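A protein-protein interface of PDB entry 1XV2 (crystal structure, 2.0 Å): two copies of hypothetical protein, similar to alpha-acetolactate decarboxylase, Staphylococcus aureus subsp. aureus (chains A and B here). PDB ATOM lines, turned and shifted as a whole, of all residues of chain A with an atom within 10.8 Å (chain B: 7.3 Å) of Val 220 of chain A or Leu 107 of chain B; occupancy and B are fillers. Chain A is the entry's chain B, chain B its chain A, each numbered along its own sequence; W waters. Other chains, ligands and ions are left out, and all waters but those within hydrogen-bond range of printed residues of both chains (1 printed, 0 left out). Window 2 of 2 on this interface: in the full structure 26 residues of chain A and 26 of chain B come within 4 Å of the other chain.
Water W1 bridges the backbone carbonyl oxygen (O) of Val 220 of chain A (2.7 Å) and the backbone carbonyl oxygen (O) of Leu 107 of chain B (3.5 Å).
The side-chain hydroxyl of Ser 108 of chain B sits close to the backbone NH of Asn 110 of chain B, at 3.0 Å. The side-chain amide oxygen of Asn 216 of chain A is in hydrogen-bond range of the backbone NH of Phe 219 of chain A, 2.8 Å away. The backbone carbonyl oxygen (O) of Phe 112 of chain B lies within hydrogen-bond range of the backbone NH (N) of Phe 205 of chain B. OD1 of Asn 204 of chain B is in hydrogen-bond range of N of Leu 107 of chain B.
O of Ala 222 of chain A is in hydrogen-bond range of ND2 of Asn 110 of chain B (2.7 Å). The backbone carbonyl oxygen (O) of Val 220 of chain A is in hydrogen-bond range of the side-chain hydroxyl (OG) of Ser 108 of chain B (2.8 Å). ND2 of Asn 110 of chain B lies within hydrogen-bond range of O of Phe 219 of chain A (2.9 Å).
Of the printed residues of chain B, Phe 219 of chain A touches Asn 110 (2.9 Å) and Leu 111 (3.7 Å). Of chain B, only Leu 107 (3.2 Å), Ser 108 (2.8 Å) and Asn 110 (3.6 Å) come within 4 Å of Val 220 of chain A. Of chain A, only Val 220 comes within 4 Å of Ser 108 of chain B. Of the printed residues of chain A, Phe 112 of chain B touches Phe 212. The nearest residue of chain B that does not touch Val 220 of chain A is Glu 109 of chain B (4.9 Å). The nearest residue of chain A that does not touch Leu 107 of chain B is Val 214 of chain A (4.04 Å). The nearest printed residue of chain B that does not touch Ile 224 of chain A is Glu 109 of chain B (5.9 Å).
Leu 111 of chain B touches Phe 212 of chain A. CE2 of Phe 212 of chain A touches CD2 of Phe 112 of chain B, 3.9 Å away. CG1 of Val 214 of chain A touches CD1 of Leu 111 of chain B, at 3.8 Å. Val 214 of chain A touches Phe 205 of chain B (CG1 to O, 3.9 Å). Leu 111 of chain B touches Phe 219 of chain A. CG1 of Val 220 of chain A touches O of Leu 107 of chain B, at 3.2 Å. O of Val 220 of chain A touches ND2 of Asn 110 of chain B, 3.6 Å away. Ile 224 of chain A touches Asn 110 of chain B.
No position is printed for both chains.
Of the 18 printed residues of chain A, 6 touch a printed residue of chain B. Among the printed residues, 11 pairs touch across the chains.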
ATOM      1  N   THR A  16       9.762   2.703  -0.310  1.00  0.00           N
ATOM      2  CA  THR A  16       8.469   3.369  -0.281  1.00  0.00           C
ATOM      3  C   THR A  16       7.875   3.430  -1.684  1.00  0.00           C
ATOM      4  O   THR A  16       6.659   3.290  -1.857  1.00  0.00           O
ATOM      5  CB  THR A  16       8.595   4.795   0.278  1.00  0.00           C
ATOM      6  OG1 THR A  16       8.913   4.727   1.673  1.00  0.00           O
ATOM      7  CG2 THR A  16       7.296   5.562   0.091  1.00  0.00           C
ATOM      8  N   LEU A  21       3.624   4.197  -3.283  1.00  0.00           N
ATOM      9  CA  LEU A  21       3.509   5.650  -3.209  1.00  0.00           C
ATOM     10  C   LEU A  21       4.259   6.265  -4.386  1.00  0.00           C
ATOM     11  O   LEU A  21       5.440   6.598  -4.279  1.00  0.00           O
ATOM     12  CB  LEU A  21       4.067   6.173  -1.882  1.00  0.00           C
ATOM     13  CG  LEU A  21       3.236   5.842  -0.634  1.00  0.00           C
ATOM     14  CD1 LEU A  21       3.377   4.367  -0.290  1.00  0.00           C
ATOM     15  CD2 LEU A  21       3.697   6.704   0.528  1.00  0.00           C
ATOM     16  N   GLU A  23       3.194   9.081  -6.031  1.00  0.00           N
ATOM     17  CA  GLU A  23       2.855  10.488  -6.207  1.00  0.00           C
ATOM     18  C   GLU A  23       4.108  11.352  -6.320  1.00  0.00           C
ATOM     19  O   GLU A  23       5.109  11.099  -5.652  1.00  0.00           O
ATOM     20  CB  GLU A  23       2.009  10.983  -5.034  1.00  0.00           C
ATOM     21  CG  GLU A  23       0.532  10.658  -5.146  1.00  0.00           C
ATOM     22  CD  GLU A  23      -0.268  11.204  -3.979  1.00  0.00           C
ATOM     23  OE1 GLU A  23      -0.113  12.402  -3.658  1.00  0.00           O
ATOM     24  OE2 GLU A  23      -1.055  10.438  -3.383  1.00  0.00           O
ATOM     25  N   THR A  25       6.330  14.196  -5.413  1.00  0.00           N
ATOM     26  CA  THR A  25       6.449  15.041  -4.231  1.00  0.00           C
ATOM     27  C   THR A  25       7.561  16.080  -4.303  1.00  0.00           C
ATOM     28  O   THR A  25       7.736  16.879  -3.383  1.00  0.00           O
ATOM     29  CB  THR A  25       6.661  14.183  -2.980  1.00  0.00           C
ATOM     30  OG1 THR A  25       7.798  13.334  -3.177  1.00  0.00           O
ATOM     31  CG2 THR A  25       5.433  13.328  -2.712  1.00  0.00           C
ATOM     32  N   PHE A 212      12.477  13.946   3.050  1.00  0.00           N
ATOM     33  CA  PHE A 212      11.139  13.357   3.145  1.00  0.00           C
ATOM     34  C   PHE A 212      10.052  14.351   2.731  1.00  0.00           C
ATOM     35  O   PHE A 212      10.167  15.550   2.984  1.00  0.00           O
ATOM     36  CB  PHE A 212      10.869  12.918   4.585  1.00  0.00           C
ATOM     37  CG  PHE A 212      11.701  11.754   5.037  1.00  0.00           C
ATOM     38  CD1 PHE A 212      11.322  10.450   4.730  1.00  0.00           C
ATOM     39  CD2 PHE A 212      12.855  11.959   5.791  1.00  0.00           C
ATOM     40  CE1 PHE A 212      12.077   9.362   5.169  1.00  0.00           C
ATOM     41  CE2 PHE A 212      13.623  10.875   6.237  1.00  0.00           C
ATOM     42  CZ  PHE A 212      13.230   9.575   5.926  1.00  0.00           C
ATOM     43  N   PRO A 213       8.976  13.860   2.095  1.00  0.00           N
ATOM     44  CA  PRO A 213       7.874  14.726   1.657  1.00  0.00           C
ATOM     45  C   PRO A 213       6.867  14.969   2.786  1.00  0.00           C
ATOM     46  O   PRO A 213       5.739  14.477   2.744  1.00  0.00           O
ATOM     47  CB  PRO A 213       7.275  13.941   0.500  1.00  0.00           C
ATOM     48  CG  PRO A 213       7.406  12.529   0.983  1.00  0.00           C
ATOM     49  CD  PRO A 213       8.815  12.496   1.556  1.00  0.00           C
ATOM     50  N   VAL A 214       7.282  15.739   3.786  1.00  0.00           N
ATOM     51  CA  VAL A 214       6.440  16.035   4.941  1.00  0.00           C
ATOM     52  C   VAL A 214       5.127  16.746   4.619  1.00  0.00           C
ATOM     53  O   VAL A 214       4.251  16.843   5.480  1.00  0.00           O
ATOM     54  CB  VAL A 214       7.205  16.880   5.982  1.00  0.00           C
ATOM     55  CG1 VAL A 214       8.356  16.075   6.562  1.00  0.00           C
ATOM     56  CG2 VAL A 214       7.726  18.153   5.336  1.00  0.00           C
ATOM     57  N   ASN A 215       4.990  17.239   3.391  1.00  0.00           N
ATOM     58  CA  ASN A 215       3.775  17.942   2.987  1.00  0.00           C
ATOM     59  C   ASN A 215       2.862  17.096   2.111  1.00  0.00           C
ATOM     60  O   ASN A 215       1.820  17.568   1.657  1.00  0.00           O
ATOM     61  CB  ASN A 215       4.126  19.234   2.243  1.00  0.00           C
ATOM     62  CG  ASN A 215       4.839  20.241   3.120  1.00  0.00           C
ATOM     63  OD1 ASN A 215       4.358  20.590   4.199  1.00  0.00           O
ATOM     64  ND2 ASN A 215       5.992  20.718   2.660  1.00  0.00           N
ATOM     65  N   ASN A 216       3.254  15.851   1.864  1.00  0.00           N
ATOM     66  CA  ASN A 216       2.450  14.955   1.042  1.00  0.00           C
ATOM     67  C   ASN A 216       1.511  14.152   1.941  1.00  0.00           C
ATOM     68  O   ASN A 216       1.912  13.160   2.549  1.00  0.00           O
ATOM     69  CB  ASN A 216       3.360  14.019   0.241  1.00  0.00           C
ATOM     70  CG  ASN A 216       2.586  13.100  -0.682  1.00  0.00           C
ATOM     71  OD1 ASN A 216       2.049  12.078  -0.256  1.00  0.00           O
ATOM     72  ND2 ASN A 216       2.516  13.467  -1.956  1.00  0.00           N
ATOM     73  N   GLU A 217       0.261  14.597   2.020  1.00  0.00           N
ATOM     74  CA  GLU A 217      -0.747  13.944   2.851  1.00  0.00           C
ATOM     75  C   GLU A 217      -0.734  12.427   2.725  1.00  0.00           C
ATOM     76  O   GLU A 217      -0.760  11.715   3.732  1.00  0.00           O
ATOM     77  CB  GLU A 217      -2.144  14.476   2.509  1.00  0.00           C
ATOM     78  CG  GLU A 217      -2.331  15.957   2.811  1.00  0.00           C
ATOM     79  CD  GLU A 217      -3.740  16.452   2.515  1.00  0.00           C
ATOM     80  OE1 GLU A 217      -4.137  16.464   1.328  1.00  0.00           O
ATOM     81  OE2 GLU A 217      -4.451  16.828   3.472  1.00  0.00           O
ATOM     82  N   THR A 218      -0.692  11.931   1.494  1.00  0.00           N
ATOM     83  CA  THR A 218      -0.678  10.492   1.265  1.00  0.00           C
ATOM     84  C   THR A 218       0.448   9.837   2.051  1.00  0.00           C
ATOM     85  O   THR A 218       0.204   8.977   2.898  1.00  0.00           O
ATOM     86  CB  THR A 218      -0.492  10.163  -0.219  1.00  0.00           C
ATOM     87  OG1 THR A 218      -1.531  10.793  -0.976  1.00  0.00           O
ATOM     88  CG2 THR A 218      -0.546   8.656  -0.438  1.00  0.00           C
ATOM     89  N   PHE A 219       1.680  10.251   1.769  1.00  0.00           N
ATOM     90  CA  PHE A 219       2.843   9.700   2.455  1.00  0.00           C
ATOM     91  C   PHE A 219       2.697   9.817   3.968  1.00  0.00           C
ATOM     92  O   PHE A 219       2.985   8.877   4.706  1.00  0.00           O
ATOM     93  CB  PHE A 219       4.120  10.428   2.024  1.00  0.00           C
ATOM     94  CG  PHE A 219       5.350   9.967   2.758  1.00  0.00           C
ATOM     95  CD1 PHE A 219       5.924   8.734   2.475  1.00  0.00           C
ATOM     96  CD2 PHE A 219       5.901  10.745   3.767  1.00  0.00           C
ATOM     97  CE1 PHE A 219       7.033   8.277   3.190  1.00  0.00           C
ATOM     98  CE2 PHE A 219       7.010  10.299   4.492  1.00  0.00           C
ATOM     99  CZ  PHE A 219       7.574   9.062   4.201  1.00  0.00           C
ATOM    100  N   VAL A 220       2.255  10.982   4.423  1.00  0.00           N
ATOM    101  CA  VAL A 220       2.080  11.232   5.846  1.00  0.00           C
ATOM    102  C   VAL A 220       1.103  10.273   6.527  1.00  0.00           C
ATOM    103  O   VAL A 220       1.436   9.666   7.543  1.00  0.00           O
ATOM    104  CB  VAL A 220       1.598  12.672   6.091  1.00  0.00           C
ATOM    105  CG1 VAL A 220       1.307  12.882   7.572  1.00  0.00           C
ATOM    106  CG2 VAL A 220       2.652  13.653   5.608  1.00  0.00           C
ATOM    107  N   LYS A 221      -0.095  10.136   5.960  1.00  0.00           N
ATOM    108  CA  LYS A 221      -1.128   9.273   6.532  1.00  0.00           C
ATOM    109  C   LYS A 221      -1.078   7.821   6.071  1.00  0.00           C
ATOM    110  O   LYS A 221      -1.773   6.967   6.619  1.00  0.00           O
ATOM    111  CB  LYS A 221      -2.514   9.842   6.218  1.00  0.00           C
ATOM    112  CG  LYS A 221      -2.759  11.237   6.764  1.00  0.00           C
ATOM    113  CD  LYS A 221      -4.174  11.704   6.438  1.00  0.00           C
ATOM    114  CE  LYS A 221      -4.435  13.100   6.974  1.00  0.00           C
ATOM    115  NZ  LYS A 221      -3.539  14.112   6.349  1.00  0.00           N
ATOM    116  N   ALA A 222      -0.258   7.533   5.072  1.00  0.00           N
ATOM    117  CA  ALA A 222      -0.166   6.177   4.553  1.00  0.00           C
ATOM    118  C   ALA A 222       0.374   5.151   5.546  1.00  0.00           C
ATOM    119  O   ALA A 222       1.219   5.460   6.389  1.00  0.00           O
ATOM    120  CB  ALA A 222       0.692   6.166   3.296  1.00  0.00           C
ATOM    121  N   LYS A 223      -0.146   3.930   5.448  1.00  0.00           N
ATOM    122  CA  LYS A 223       0.306   2.819   6.277  1.00  0.00           C
ATOM    123  C   LYS A 223       1.036   1.943   5.272  1.00  0.00           C
ATOM    124  O   LYS A 223       0.464   1.013   4.703  1.00  0.00           O
ATOM    125  CB  LYS A 223      -0.870   2.045   6.876  1.00  0.00           C
ATOM    126  CG  LYS A 223      -0.424   0.846   7.704  1.00  0.00           C
ATOM    127  CD  LYS A 223      -1.594   0.022   8.209  1.00  0.00           C
ATOM    128  CE  LYS A 223      -1.109  -1.213   8.958  1.00  0.00           C
ATOM    129  NZ  LYS A 223      -2.236  -2.062   9.438  1.00  0.00           N
ATOM    130  N   ILE A 224       2.302   2.268   5.049  1.00  0.00           N
ATOM    131  CA  ILE A 224       3.137   1.573   4.080  1.00  0.00           C
ATOM    132  C   ILE A 224       3.455   0.121   4.414  1.00  0.00           C
ATOM    133  O   ILE A 224       3.922  -0.187   5.511  1.00  0.00           O
ATOM    134  CB  ILE A 224       4.458   2.334   3.893  1.00  0.00           C
ATOM    135  CG1 ILE A 224       4.171   3.837   3.816  1.00  0.00           C
ATOM    136  CG2 ILE A 224       5.158   1.854   2.638  1.00  0.00           C
ATOM    137  CD1 ILE A 224       5.407   4.705   3.746  1.00  0.00           C
ATOM    138  N   TYR A 226       5.741  -3.045   3.613  1.00  0.00           N
ATOM    139  CA  TYR A 226       7.027  -3.400   3.030  1.00  0.00           C
ATOM    140  C   TYR A 226       7.226  -4.902   2.905  1.00  0.00           C
ATOM    141  O   TYR A 226       8.316  -5.361   2.566  1.00  0.00           O
ATOM    142  CB  TYR A 226       8.154  -2.808   3.878  1.00  0.00           C
ATOM    143  CG  TYR A 226       8.173  -1.298   3.895  1.00  0.00           C
ATOM    144  CD1 TYR A 226       8.561  -0.576   2.769  1.00  0.00           C
ATOM    145  CD2 TYR A 226       7.808  -0.588   5.040  1.00  0.00           C
ATOM    146  CE1 TYR A 226       8.591   0.815   2.780  1.00  0.00           C
ATOM    147  CE2 TYR A 226       7.832   0.807   5.061  1.00  0.00           C
ATOM    148  CZ  TYR A 226       8.227   1.500   3.927  1.00  0.00           C
ATOM    149  OH  TYR A 226       8.268   2.877   3.939  1.00  0.00           O
ATOM    150  N   SER B  85       7.768  20.911  17.942  1.00  0.00           N
ATOM    151  CA  SER B  85       6.691  21.370  17.075  1.00  0.00           C
ATOM    152  C   SER B  85       5.348  21.087  17.743  1.00  0.00           C
ATOM    153  O   SER B  85       4.304  21.558  17.290  1.00  0.00           O
ATOM    154  CB  SER B  85       6.766  20.680  15.713  1.00  0.00           C
ATOM    155  OG  SER B  85       6.838  19.277  15.853  1.00  0.00           O
ATOM    156  N   LYS B  86       5.387  20.320  18.829  1.00  0.00           N
ATOM    157  CA  LYS B  86       4.184  19.985  19.577  1.00  0.00           C
ATOM    158  C   LYS B  86       4.534  19.661  21.025  1.00  0.00           C
ATOM    159  O   LYS B  86       5.540  19.005  21.299  1.00  0.00           O
ATOM    160  CB  LYS B  86       3.459  18.795  18.934  1.00  0.00           C
ATOM    161  CG  LYS B  86       2.172  18.412  19.655  1.00  0.00           C
ATOM    162  CD  LYS B  86       1.409  17.305  18.941  1.00  0.00           C
ATOM    163  CE  LYS B  86       0.760  17.800  17.656  1.00  0.00           C
ATOM    164  NZ  LYS B  86      -0.010  16.715  16.970  1.00  0.00           N
ATOM    165  N   ILE B 102       2.404   9.328  21.836  1.00  0.00           N
ATOM    166  CA  ILE B 102       3.373   9.951  20.949  1.00  0.00           C
ATOM    167  C   ILE B 102       3.084   9.525  19.512  1.00  0.00           C
ATOM    168  O   ILE B 102       3.172  10.331  18.588  1.00  0.00           O
ATOM    169  CB  ILE B 102       4.817   9.560  21.354  1.00  0.00           C
ATOM    170  CG1 ILE B 102       5.089  10.047  22.782  1.00  0.00           C
ATOM    171  CG2 ILE B 102       5.821  10.179  20.391  1.00  0.00           C
ATOM    172  CD1 ILE B 102       6.406   9.593  23.368  1.00  0.00           C
ATOM    173  N   LYS B 103       2.716   8.262  19.330  1.00  0.00           N
ATOM    174  CA  LYS B 103       2.399   7.747  18.002  1.00  0.00           C
ATOM    175  C   LYS B 103       1.185   8.476  17.431  1.00  0.00           C
ATOM    176  O   LYS B 103       1.038   8.605  16.215  1.00  0.00           O
ATOM    177  CB  LYS B 103       2.116   6.244  18.073  1.00  0.00           C
ATOM    178  CG  LYS B 103       3.337   5.396  18.402  1.00  0.00           C
ATOM    179  CD  LYS B 103       4.227   5.191  17.186  1.00  0.00           C
ATOM    180  CE  LYS B 103       3.515   4.336  16.142  1.00  0.00           C
ATOM    181  NZ  LYS B 103       4.377   4.004  14.979  1.00  0.00           N
ATOM    182  N   ASN B 104       0.321   8.959  18.319  1.00  0.00           N
ATOM    183  CA  ASN B 104      -0.880   9.685  17.912  1.00  0.00           C
ATOM    184  C   ASN B 104      -0.590  11.144  17.582  1.00  0.00           C
ATOM    185  O   ASN B 104      -1.171  11.704  16.652  1.00  0.00           O
ATOM    186  CB  ASN B 104      -1.931   9.641  19.029  1.00  0.00           C
ATOM    187  CG  ASN B 104      -2.544   8.264  19.209  1.00  0.00           C
ATOM    188  OD1 ASN B 104      -3.198   7.994  20.219  1.00  0.00           O
ATOM    189  ND2 ASN B 104      -2.349   7.390  18.226  1.00  0.00           N
ATOM    190  N   GLU B 105       0.308  11.755  18.351  1.00  0.00           N
ATOM    191  CA  GLU B 105       0.647  13.159  18.164  1.00  0.00           C
ATOM    192  C   GLU B 105       1.722  13.468  17.124  1.00  0.00           C
ATOM    193  O   GLU B 105       1.776  14.583  16.608  1.00  0.00           O
ATOM    194  CB  GLU B 105       1.036  13.777  19.510  1.00  0.00           C
ATOM    195  CG  GLU B 105      -0.068  13.694  20.554  1.00  0.00           C
ATOM    196  CD  GLU B 105      -1.395  14.239  20.040  1.00  0.00           C
ATOM    197  OE1 GLU B 105      -1.433  15.410  19.606  1.00  0.00           O
ATOM    198  OE2 GLU B 105      -2.400  13.496  20.070  1.00  0.00           O
ATOM    199  N   MET B 106       2.579  12.500  16.814  1.00  0.00           N
ATOM    200  CA  MET B 106       3.619  12.736  15.816  1.00  0.00           C
ATOM    201  C   MET B 106       2.973  12.968  14.454  1.00  0.00           C
ATOM    202  O   MET B 106       1.840  12.543  14.219  1.00  0.00           O
ATOM    203  CB  MET B 106       4.576  11.544  15.730  1.00  0.00           C
ATOM    204  CG  MET B 106       3.927  10.240  15.307  1.00  0.00           C
ATOM    205  SD  MET B 106       5.227   8.843  14.971  1.00  0.00           S
ATOM    206  CE  MET B 106       5.956   8.681  16.746  1.00  0.00           C
ATOM    207  N   LEU B 107       3.693  13.644  13.562  1.00  0.00           N
ATOM    208  CA  LEU B 107       3.185  13.936  12.226  1.00  0.00           C
ATOM    209  C   LEU B 107       2.957  12.677  11.401  1.00  0.00           C
ATOM    210  O   LEU B 107       1.972  12.573  10.669  1.00  0.00           O
ATOM    211  CB  LEU B 107       4.151  14.856  11.475  1.00  0.00           C
ATOM    212  CG  LEU B 107       3.854  15.042   9.981  1.00  0.00           C
ATOM    213  CD1 LEU B 107       2.461  15.628   9.795  1.00  0.00           C
ATOM    214  CD2 LEU B 107       4.907  15.954   9.361  1.00  0.00           C
ATOM    215  N   SER B 108       3.872  11.721  11.519  1.00  0.00           N
ATOM    216  CA  SER B 108       3.764  10.481  10.768  1.00  0.00           C
ATOM    217  C   SER B 108       4.751   9.429  11.249  1.00  0.00           C
ATOM    218  O   SER B 108       5.901   9.738  11.565  1.00  0.00           O
ATOM    219  CB  SER B 108       4.010  10.746   9.285  1.00  0.00           C
ATOM    220  OG  SER B 108       4.023   9.535   8.555  1.00  0.00           O
ATOM    221  N   GLU B 109       4.295   8.181  11.301  1.00  0.00           N
ATOM    222  CA  GLU B 109       5.158   7.093  11.721  1.00  0.00           C
ATOM    223  C   GLU B 109       6.015   6.659  10.538  1.00  0.00           C
ATOM    224  O   GLU B 109       6.751   5.681  10.620  1.00  0.00           O
ATOM    225  CB  GLU B 109       4.333   5.911  12.241  1.00  0.00           C
ATOM    226  CG  GLU B 109       3.276   5.404  11.282  1.00  0.00           C
ATOM    227  CD  GLU B 109       2.700   4.066  11.712  1.00  0.00           C
ATOM    228  OE1 GLU B 109       2.539   3.849  12.935  1.00  0.00           O
ATOM    229  OE2 GLU B 109       2.395   3.238  10.826  1.00  0.00           O
ATOM    230  N   ASN B 110       5.903   7.387   9.430  1.00  0.00           N
ATOM    231  CA  ASN B 110       6.695   7.092   8.240  1.00  0.00           C
ATOM    232  C   ASN B 110       7.884   8.062   8.200  1.00  0.00           C
ATOM    233  O   ASN B 110       8.667   8.076   7.250  1.00  0.00           O
ATOM    234  CB  ASN B 110       5.853   7.260   6.973  1.00  0.00           C
ATOM    235  CG  ASN B 110       4.676   6.305   6.918  1.00  0.00           C
ATOM    236  OD1 ASN B 110       4.832   5.092   7.078  1.00  0.00           O
ATOM    237  ND2 ASN B 110       3.487   6.849   6.676  1.00  0.00           N
ATOM    238  N   LEU B 111       7.999   8.871   9.249  1.00  0.00           N
ATOM    239  CA  LEU B 111       9.068   9.855   9.375  1.00  0.00           C
ATOM    240  C   LEU B 111       9.843   9.651  10.665  1.00  0.00           C
ATOM    241  O   LEU B 111       9.377   8.983  11.590  1.00  0.00           O
ATOM    242  CB  LEU B 111       8.489  11.270   9.410  1.00  0.00           C
ATOM    243  CG  LEU B 111       7.815  11.838   8.164  1.00  0.00           C
ATOM    244  CD1 LEU B 111       7.081  13.120   8.536  1.00  0.00           C
ATOM    245  CD2 LEU B 111       8.855  12.100   7.089  1.00  0.00           C
ATOM    246  N   PHE B 112      11.035  10.233  10.715  1.00  0.00           N
ATOM    247  CA  PHE B 112      11.861  10.185  11.911  1.00  0.00           C
ATOM    248  C   PHE B 112      11.287  11.295  12.786  1.00  0.00           C
ATOM    249  O   PHE B 112      10.713  12.258  12.272  1.00  0.00           O
ATOM    250  CB  PHE B 112      13.312  10.532  11.572  1.00  0.00           C
ATOM    251  CG  PHE B 112      14.122   9.375  11.062  1.00  0.00           C
ATOM    252  CD1 PHE B 112      14.772   8.525  11.947  1.00  0.00           C
ATOM    253  CD2 PHE B 112      14.270   9.163   9.695  1.00  0.00           C
ATOM    254  CE1 PHE B 112      15.564   7.482  11.479  1.00  0.00           C
ATOM    255  CE2 PHE B 112      15.059   8.121   9.216  1.00  0.00           C
ATOM    256  CZ  PHE B 112      15.708   7.282  10.111  1.00  0.00           C
ATOM    257  N   SER B 113      11.439  11.167  14.098  1.00  0.00           N
ATOM    258  CA  SER B 113      10.957  12.189  15.022  1.00  0.00           C
ATOM    259  C   SER B 113      11.769  12.141  16.305  1.00  0.00           C
ATOM    260  O   SER B 113      12.389  11.127  16.626  1.00  0.00           O
ATOM    261  CB  SER B 113       9.473  11.982  15.344  1.00  0.00           C
ATOM    262  OG  SER B 113       9.252  10.712  15.935  1.00  0.00           O
ATOM    263  N   ILE B 202       7.554  16.918  21.024  1.00  0.00           N
ATOM    264  CA  ILE B 202       7.868  16.160  19.821  1.00  0.00           C
ATOM    265  C   ILE B 202       8.366  17.074  18.708  1.00  0.00           C
ATOM    266  O   ILE B 202       7.995  18.249  18.637  1.00  0.00           O
ATOM    267  CB  ILE B 202       6.627  15.410  19.291  1.00  0.00           C
ATOM    268  CG1 ILE B 202       6.047  14.512  20.380  1.00  0.00           C
ATOM    269  CG2 ILE B 202       7.006  14.561  18.086  1.00  0.00           C
ATOM    270  CD1 ILE B 202       4.795  13.766  19.948  1.00  0.00           C
ATOM    271  N   GLN B 203       9.213  16.523  17.845  1.00  0.00           N
ATOM    272  CA  GLN B 203       9.741  17.252  16.701  1.00  0.00           C
ATOM    273  C   GLN B 203       9.775  16.287  15.522  1.00  0.00           C
ATOM    274  O   GLN B 203      10.382  15.219  15.607  1.00  0.00           O
ATOM    275  CB  GLN B 203      11.150  17.774  16.981  1.00  0.00           C
ATOM    276  CG  GLN B 203      11.726  18.574  15.817  1.00  0.00           C
ATOM    277  CD  GLN B 203      13.147  19.044  16.058  1.00  0.00           C
ATOM    278  OE1 GLN B 203      13.699  19.806  15.265  1.00  0.00           O
ATOM    279  NE2 GLN B 203      13.750  18.587  17.151  1.00  0.00           N
ATOM    280  N   ASN B 204       9.111  16.657  14.432  1.00  0.00           N
ATOM    281  CA  ASN B 204       9.068  15.819  13.241  1.00  0.00           C
ATOM    282  C   ASN B 204      10.170  16.257  12.277  1.00  0.00           C
ATOM    283  O   ASN B 204      10.336  17.447  12.019  1.00  0.00           O
ATOM    284  CB  ASN B 204       7.694  15.935  12.578  1.00  0.00           C
ATOM    285  CG  ASN B 204       6.558  15.665  13.552  1.00  0.00           C
ATOM    286  OD1 ASN B 204       6.391  14.545  14.040  1.00  0.00           O
ATOM    287  ND2 ASN B 204       5.777  16.696  13.846  1.00  0.00           N
ATOM    288  N   PHE B 205      10.915  15.292  11.745  1.00  0.00           N
ATOM    289  CA  PHE B 205      12.021  15.587  10.838  1.00  0.00           C
ATOM    290  C   PHE B 205      11.691  15.459   9.357  1.00  0.00           C
ATOM    291  O   PHE B 205      11.020  14.522   8.928  1.00  0.00           O
ATOM    292  CB  PHE B 205      13.225  14.694  11.174  1.00  0.00           C
ATOM    293  CG  PHE B 205      13.823  14.968  12.529  1.00  0.00           C
ATOM    294  CD1 PHE B 205      14.383  16.210  12.819  1.00  0.00           C
ATOM    295  CD2 PHE B 205      13.799  13.995  13.523  1.00  0.00           C
ATOM    296  CE1 PHE B 205      14.909  16.481  14.087  1.00  0.00           C
ATOM    297  CE2 PHE B 205      14.323  14.255  14.795  1.00  0.00           C
ATOM    298  CZ  PHE B 205      14.878  15.499  15.076  1.00  0.00           C
HETATM  299  O   HOH W   1       0.159   9.663   9.978  1.00  0.00           O
